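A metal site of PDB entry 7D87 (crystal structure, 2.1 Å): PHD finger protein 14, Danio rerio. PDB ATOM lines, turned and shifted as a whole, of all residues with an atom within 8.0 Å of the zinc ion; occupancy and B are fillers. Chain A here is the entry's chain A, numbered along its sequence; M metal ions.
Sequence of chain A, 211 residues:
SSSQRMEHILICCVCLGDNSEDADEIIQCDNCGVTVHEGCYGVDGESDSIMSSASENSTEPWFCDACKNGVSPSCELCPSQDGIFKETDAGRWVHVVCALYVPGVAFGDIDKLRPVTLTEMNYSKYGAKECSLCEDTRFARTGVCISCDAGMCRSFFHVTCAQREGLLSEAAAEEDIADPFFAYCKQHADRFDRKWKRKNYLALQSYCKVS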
ATOM      1  N   SER A  74      10.144  14.257 -18.881  1.00  0.00           N
ATOM      2  CA  SER A  74      11.175  14.139 -19.887  1.00  0.00           C
ATOM      3  C   SER A  74      11.058  15.305 -20.857  1.00  0.00           C
ATOM      4  O   SER A  74      10.024  15.974 -20.951  1.00  0.00           O
ATOM      5  CB  SER A  74      11.057  12.796 -20.609  1.00  0.00           C
ATOM      6  OG  SER A  74       9.734  12.625 -21.062  1.00  0.00           O
ATOM      7  N   CYS A  75      12.145  15.556 -21.579  1.00  0.00           N
ATOM      8  CA  CYS A  75      12.220  16.683 -22.501  1.00  0.00           C
ATOM      9  C   CYS A  75      11.839  16.218 -23.897  1.00  0.00           C
ATOM     10  O   CYS A  75      12.227  15.134 -24.335  1.00  0.00           O
ATOM     11  CB  CYS A  75      13.641  17.278 -22.486  1.00  0.00           C
ATOM     12  SG  CYS A  75      13.882  18.664 -23.592  1.00  0.00           S
ATOM     13  N   GLU A  76      11.062  17.043 -24.595  1.00  0.00           N
ATOM     14  CA  GLU A  76      10.709  16.757 -25.980  1.00  0.00           C
ATOM     15  C   GLU A  76      11.913  16.788 -26.910  1.00  0.00           C
ATOM     16  O   GLU A  76      11.838  16.271 -28.021  1.00  0.00           O
ATOM     17  CB  GLU A  76       9.662  17.765 -26.501  1.00  0.00           C
ATOM     18  CG  GLU A  76       8.304  17.681 -25.833  1.00  0.00           C
ATOM     19  CD  GLU A  76       7.632  16.343 -26.079  1.00  0.00           C
ATOM     20  OE1 GLU A  76       7.073  16.162 -27.196  1.00  0.00           O
ATOM     21  OE2 GLU A  76       7.646  15.485 -25.165  1.00  0.00           O
ATOM     22  N   LEU A  77      13.021  17.393 -26.488  1.00  0.00           N
ATOM     23  CA  LEU A  77      14.136  17.669 -27.390  1.00  0.00           C
ATOM     24  C   LEU A  77      15.423  16.907 -27.057  1.00  0.00           C
ATOM     25  O   LEU A  77      16.423  17.100 -27.766  1.00  0.00           O
ATOM     26  CB  LEU A  77      14.415  19.184 -27.415  1.00  0.00           C
ATOM     27  CG  LEU A  77      13.291  20.101 -27.903  1.00  0.00           C
ATOM     28  CD1 LEU A  77      13.648  21.562 -27.667  1.00  0.00           C
ATOM     29  CD2 LEU A  77      13.028  19.872 -29.364  1.00  0.00           C
ATOM     30  N   CYS A  78      15.441  16.072 -26.030  1.00  0.00           N
ATOM     31  CA  CYS A  78      16.664  15.368 -25.650  1.00  0.00           C
ATOM     32  C   CYS A  78      16.294  14.263 -24.679  1.00  0.00           C
ATOM     33  O   CYS A  78      15.172  14.268 -24.155  1.00  0.00           O
ATOM     34  CB  CYS A  78      17.694  16.331 -25.018  1.00  0.00           C
ATOM     35  SG  CYS A  78      17.386  16.717 -23.274  1.00  0.00           S
ATOM     36  N   PRO A  79      17.204  13.326 -24.429  1.00  0.00           N
ATOM     37  CA  PRO A  79      16.920  12.195 -23.524  1.00  0.00           C
ATOM     38  C   PRO A  79      17.259  12.420 -22.066  1.00  0.00           C
ATOM     39  O   PRO A  79      16.983  11.534 -21.247  1.00  0.00           O
ATOM     40  CB  PRO A  79      17.802  11.077 -24.087  1.00  0.00           C
ATOM     41  CG  PRO A  79      19.006  11.795 -24.596  1.00  0.00           C
ATOM     42  CD  PRO A  79      18.458  13.103 -25.177  1.00  0.00           C
ATOM     43  N   SER A  80      17.821  13.565 -21.703  1.00  0.00           N
ATOM     44  CA  SER A  80      18.242  13.786 -20.322  1.00  0.00           C
ATOM     45  C   SER A  80      17.042  14.062 -19.416  1.00  0.00           C
ATOM     46  O   SER A  80      16.070  14.703 -19.825  1.00  0.00           O
ATOM     47  CB  SER A  80      19.220  14.959 -20.257  1.00  0.00           C
ATOM     48  OG  SER A  80      19.538  15.264 -18.916  1.00  0.00           O
ATOM     49  N   GLN A  81      17.141  13.595 -18.171  1.00  0.00           N
ATOM     50  CA  GLN A  81      16.094  13.755 -17.166  1.00  0.00           C
ATOM     51  C   GLN A  81      16.428  14.801 -16.116  1.00  0.00           C
ATOM     52  O   GLN A  81      15.564  15.141 -15.309  1.00  0.00           O
ATOM     53  CB  GLN A  81      15.816  12.420 -16.458  1.00  0.00           C
ATOM     54  CG  GLN A  81      15.398  11.297 -17.367  1.00  0.00           C
ATOM     55  CD  GLN A  81      13.946  11.376 -17.742  1.00  0.00           C
ATOM     56  OE1 GLN A  81      13.594  11.484 -18.915  1.00  0.00           O
ATOM     57  NE2 GLN A  81      13.073  11.301 -16.731  1.00  0.00           N
ATOM     58  N   ASP A  82      17.666  15.283 -16.079  1.00  0.00           N
ATOM     59  CA  ASP A  82      18.106  16.253 -15.105  1.00  0.00           C
ATOM     60  C   ASP A  82      17.901  17.675 -15.645  1.00  0.00           C
ATOM     61  O   ASP A  82      17.510  17.874 -16.800  1.00  0.00           O
ATOM     62  CB  ASP A  82      19.571  16.011 -14.734  1.00  0.00           C
ATOM     63  CG  ASP A  82      19.876  14.528 -14.508  1.00  0.00           C
ATOM     64  OD1 ASP A  82      19.387  13.954 -13.507  1.00  0.00           O
ATOM     65  OD2 ASP A  82      20.589  13.942 -15.362  1.00  0.00           O
ATOM     66  N   ILE A  84      16.356  21.753 -15.480  1.00  0.00           N
ATOM     67  CA  ILE A  84      15.131  22.455 -15.170  1.00  0.00           C
ATOM     68  C   ILE A  84      14.309  22.638 -16.441  1.00  0.00           C
ATOM     69  O   ILE A  84      14.859  22.808 -17.535  1.00  0.00           O
ATOM     70  CB  ILE A  84      15.444  23.787 -14.459  1.00  0.00           C
ATOM     71  CG1 ILE A  84      14.230  24.274 -13.673  1.00  0.00           C
ATOM     72  CG2 ILE A  84      16.003  24.835 -15.406  1.00  0.00           C
ATOM     73  CD1 ILE A  84      14.547  25.370 -12.677  1.00  0.00           C
ATOM     74  N   PHE A  85      12.974  22.551 -16.294  1.00  0.00           N
ATOM     75  CA  PHE A  85      12.035  22.392 -17.394  1.00  0.00           C
ATOM     76  C   PHE A  85      11.016  23.518 -17.436  1.00  0.00           C
ATOM     77  O   PHE A  85      10.740  24.176 -16.435  1.00  0.00           O
ATOM     78  CB  PHE A  85      11.261  21.067 -17.279  1.00  0.00           C
ATOM     79  CG  PHE A  85      12.107  19.825 -17.471  1.00  0.00           C
ATOM     80  CD1 PHE A  85      12.844  19.296 -16.427  1.00  0.00           C
ATOM     81  CD2 PHE A  85      12.121  19.167 -18.693  1.00  0.00           C
ATOM     82  CE1 PHE A  85      13.606  18.137 -16.598  1.00  0.00           C
ATOM     83  CE2 PHE A  85      12.882  18.012 -18.886  1.00  0.00           C
ATOM     84  CZ  PHE A  85      13.622  17.499 -17.817  1.00  0.00           C
ATOM     85  N   TRP A  93       6.953  18.993 -22.046  1.00  0.00           N
ATOM     86  CA  TRP A  93       8.003  19.674 -21.301  1.00  0.00           C
ATOM     87  C   TRP A  93       9.285  19.715 -22.124  1.00  0.00           C
ATOM     88  O   TRP A  93       9.570  18.789 -22.896  1.00  0.00           O
ATOM     89  CB  TRP A  93       8.250  18.999 -19.948  1.00  0.00           C
ATOM     90  CG  TRP A  93       7.054  18.988 -19.088  1.00  0.00           C
ATOM     91  CD1 TRP A  93       6.036  18.083 -19.102  1.00  0.00           C
ATOM     92  CD2 TRP A  93       6.709  19.954 -18.086  1.00  0.00           C
ATOM     93  NE1 TRP A  93       5.094  18.420 -18.175  1.00  0.00           N
ATOM     94  CE2 TRP A  93       5.480  19.567 -17.545  1.00  0.00           C
ATOM     95  CE3 TRP A  93       7.334  21.117 -17.599  1.00  0.00           C
ATOM     96  CZ2 TRP A  93       4.853  20.287 -16.533  1.00  0.00           C
ATOM     97  CZ3 TRP A  93       6.713  21.829 -16.607  1.00  0.00           C
ATOM     98  CH2 TRP A  93       5.486  21.414 -16.080  1.00  0.00           C
ATOM     99  N   VAL A  94      10.029  20.810 -21.977  1.00  0.00           N
ATOM    100  CA  VAL A  94      11.349  20.966 -22.576  1.00  0.00           C
ATOM    101  C   VAL A  94      12.285  21.625 -21.565  1.00  0.00           C
ATOM    102  O   VAL A  94      11.865  22.429 -20.732  1.00  0.00           O
ATOM    103  CB  VAL A  94      11.295  21.814 -23.875  1.00  0.00           C
ATOM    104  CG1 VAL A  94      10.340  21.205 -24.876  1.00  0.00           C
ATOM    105  CG2 VAL A  94      10.904  23.262 -23.567  1.00  0.00           C
ATOM    106  N   HIS A  95      13.558  21.245 -21.612  1.00  0.00           N
ATOM    107  CA  HIS A  95      14.573  22.004 -20.893  1.00  0.00           C
ATOM    108  C   HIS A  95      14.570  23.452 -21.362  1.00  0.00           C
ATOM    109  O   HIS A  95      14.409  23.734 -22.557  1.00  0.00           O
ATOM    110  CB  HIS A  95      15.967  21.441 -21.121  1.00  0.00           C
ATOM    111  CG  HIS A  95      16.187  20.098 -20.510  1.00  0.00           C
ATOM    112  ND1 HIS A  95      16.255  18.941 -21.266  1.00  0.00           N
ATOM    113  CD2 HIS A  95      16.380  19.731 -19.227  1.00  0.00           C
ATOM    114  CE1 HIS A  95      16.471  17.913 -20.456  1.00  0.00           C
ATOM    115  NE2 HIS A  95      16.543  18.371 -19.214  1.00  0.00           N
ATOM    116  N   VAL A  96      14.779  24.371 -20.419  1.00  0.00           N
ATOM    117  CA  VAL A  96      15.089  25.755 -20.795  1.00  0.00           C
ATOM    118  C   VAL A  96      16.286  25.779 -21.740  1.00  0.00           C
ATOM    119  O   VAL A  96      16.293  26.470 -22.765  1.00  0.00           O
ATOM    120  CB  VAL A  96      15.353  26.603 -19.537  1.00  0.00           C
ATOM    121  CG1 VAL A  96      15.836  28.000 -19.941  1.00  0.00           C
ATOM    122  CG2 VAL A  96      14.102  26.700 -18.696  1.00  0.00           C
ATOM    123  N   VAL A  97      17.322  25.012 -21.398  1.00  0.00           N
ATOM    124  CA  VAL A  97      18.561  25.090 -22.179  1.00  0.00           C
ATOM    125  C   VAL A  97      18.315  24.580 -23.604  1.00  0.00           C
ATOM    126  O   VAL A  97      18.777  25.193 -24.579  1.00  0.00           O
ATOM    127  CB  VAL A  97      19.700  24.338 -21.449  1.00  0.00           C
ATOM    128  CG1 VAL A  97      19.601  22.806 -21.593  1.00  0.00           C
ATOM    129  CG2 VAL A  97      21.050  24.842 -21.874  1.00  0.00           C
ATOM    130  N   CYS A  98      17.525  23.511 -23.766  1.00  0.00           N
ATOM    131  CA  CYS A  98      17.221  23.034 -25.112  1.00  0.00           C
ATOM    132  C   CYS A  98      16.417  24.056 -25.904  1.00  0.00           C
ATOM    133  O   CYS A  98      16.687  24.297 -27.087  1.00  0.00           O
ATOM    134  CB  CYS A  98      16.453  21.709 -25.070  1.00  0.00           C
ATOM    135  SG  CYS A  98      17.465  20.290 -24.559  1.00  0.00           S
ATOM    136  N   ALA A  99      15.453  24.699 -25.250  1.00  0.00           N
ATOM    137  CA  ALA A  99      14.668  25.732 -25.915  1.00  0.00           C
ATOM    138  C   ALA A  99      15.535  26.887 -26.360  1.00  0.00           C
ATOM    139  O   ALA A  99      15.344  27.438 -27.447  1.00  0.00           O
ATOM    140  CB  ALA A  99      13.548  26.212 -24.985  1.00  0.00           C
ATOM    141  N   VAL A 102      18.065  25.275 -29.464  1.00  0.00           N
ATOM    142  CA  VAL A 102      17.541  24.630 -30.679  1.00  0.00           C
ATOM    143  C   VAL A 102      16.932  25.696 -31.574  1.00  0.00           C
ATOM    144  O   VAL A 102      16.071  26.474 -31.121  1.00  0.00           O
ATOM    145  CB  VAL A 102      16.525  23.558 -30.324  1.00  0.00           C
ATOM    146  CG1 VAL A 102      15.740  23.158 -31.568  1.00  0.00           C
ATOM    147  CG2 VAL A 102      17.243  22.330 -29.743  1.00  0.00           C
ATOM    148  N   GLY A 143      14.970  12.894 -29.692  1.00  0.00           N
ATOM    149  CA  GLY A 143      15.049  14.341 -29.578  1.00  0.00           C
ATOM    150  C   GLY A 143      15.655  15.003 -30.804  1.00  0.00           C
ATOM    151  O   GLY A 143      15.619  14.486 -31.931  1.00  0.00           O
ATOM    152  N   VAL A 144      16.250  16.176 -30.576  1.00  0.00           N
ATOM    153  CA  VAL A 144      16.743  17.044 -31.637  1.00  0.00           C
ATOM    154  C   VAL A 144      18.179  17.426 -31.297  1.00  0.00           C
ATOM    155  O   VAL A 144      18.462  17.804 -30.156  1.00  0.00           O
ATOM    156  CB  VAL A 144      15.838  18.273 -31.805  1.00  0.00           C
ATOM    157  CG1 VAL A 144      16.378  19.283 -32.829  1.00  0.00           C
ATOM    158  CG2 VAL A 144      14.416  17.817 -32.202  1.00  0.00           C
ATOM    159  N   HIS A 158      22.929  16.495 -28.906  1.00  0.00           N
ATOM    160  CA  HIS A 158      21.882  17.020 -28.039  1.00  0.00           C
ATOM    161  C   HIS A 158      22.396  18.225 -27.244  1.00  0.00           C
ATOM    162  O   HIS A 158      23.559  18.284 -26.857  1.00  0.00           O
ATOM    163  CB  HIS A 158      21.436  15.930 -27.063  1.00  0.00           C
ATOM    164  CG  HIS A 158      20.706  14.799 -27.717  1.00  0.00           C
ATOM    165  ND1 HIS A 158      21.140  13.492 -27.635  1.00  0.00           N
ATOM    166  CD2 HIS A 158      19.573  14.781 -28.455  1.00  0.00           C
ATOM    167  CE1 HIS A 158      20.309  12.714 -28.306  1.00  0.00           C
ATOM    168  NE2 HIS A 158      19.345  13.471 -28.816  1.00  0.00           N
ATOM    169  N   VAL A 159      21.503  19.197 -26.986  1.00  0.00           N
ATOM    170  CA  VAL A 159      21.946  20.387 -26.264  1.00  0.00           C
ATOM    171  C   VAL A 159      22.474  20.022 -24.870  1.00  0.00           C
ATOM    172  O   VAL A 159      23.478  20.558 -24.421  1.00  0.00           O
ATOM    173  CB  VAL A 159      20.810  21.429 -26.167  1.00  0.00           C
ATOM    174  CG1 VAL A 159      21.247  22.611 -25.319  1.00  0.00           C
ATOM    175  CG2 VAL A 159      20.396  21.920 -27.565  1.00  0.00           C
ATOM    176  N   THR A 160      21.800  19.090 -24.180  1.00  0.00           N
ATOM    177  CA  THR A 160      22.215  18.719 -22.831  1.00  0.00           C
ATOM    178  C   THR A 160      23.446  17.826 -22.818  1.00  0.00           C
ATOM    179  O   THR A 160      24.172  17.790 -21.814  1.00  0.00           O
ATOM    180  CB  THR A 160      21.077  18.007 -22.123  1.00  0.00           C
ATOM    181  OG1 THR A 160      20.466  17.102 -23.048  1.00  0.00           O
ATOM    182  CG2 THR A 160      20.054  19.021 -21.618  1.00  0.00           C
ATOM    183  N   CYS A 161      23.668  17.050 -23.888  1.00  0.00           N
ATOM    184  CA  CYS A 161      24.927  16.314 -23.984  1.00  0.00           C
ATOM    185  C   CYS A 161      26.090  17.278 -24.220  1.00  0.00           C
ATOM    186  O   CYS A 161      27.160  17.129 -23.625  1.00  0.00           O
ATOM    187  CB  CYS A 161      24.853  15.247 -25.076  1.00  0.00           C
ATOM    188  SG  CYS A 161      23.648  13.885 -24.799  1.00  0.00           S
HETATM  189 ZN    ZN M   1      16.245  18.699 -23.289  1.00  0.00          ZN
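A ring nitrogen (NE2) of His 95 sits at hydrogen-bond distance from the backbone carbonyl oxygen of Asp 82 (2.6 Å). OG1 of Thr 160 lies close to SG of Cys 78 (3.1 Å). SG of Cys 78 sits close to N of Ser 80, 3.5 Å away. SG of Cys 75 lies close to N of Leu 77, at 3.3 Å.
Within 4 Å of the zinc ion: Cys 75, Cys 78, His 95 and Cys 98. Along chain A the residues within 4 Å of the zinc ion span positions 75 to 98. The nearest printed residue that does not touch the zinc ion is Thr 160 (4.2 Å).
The zinc ion is bound by ND1 of His 95 (2.0 Å), SG of Cys 78 (2.3 Å), SG of Cys 98 (2.4 Å) and SG of Cys 75 (2.4 Å). The zinc ion has four donor atoms within binding distance.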
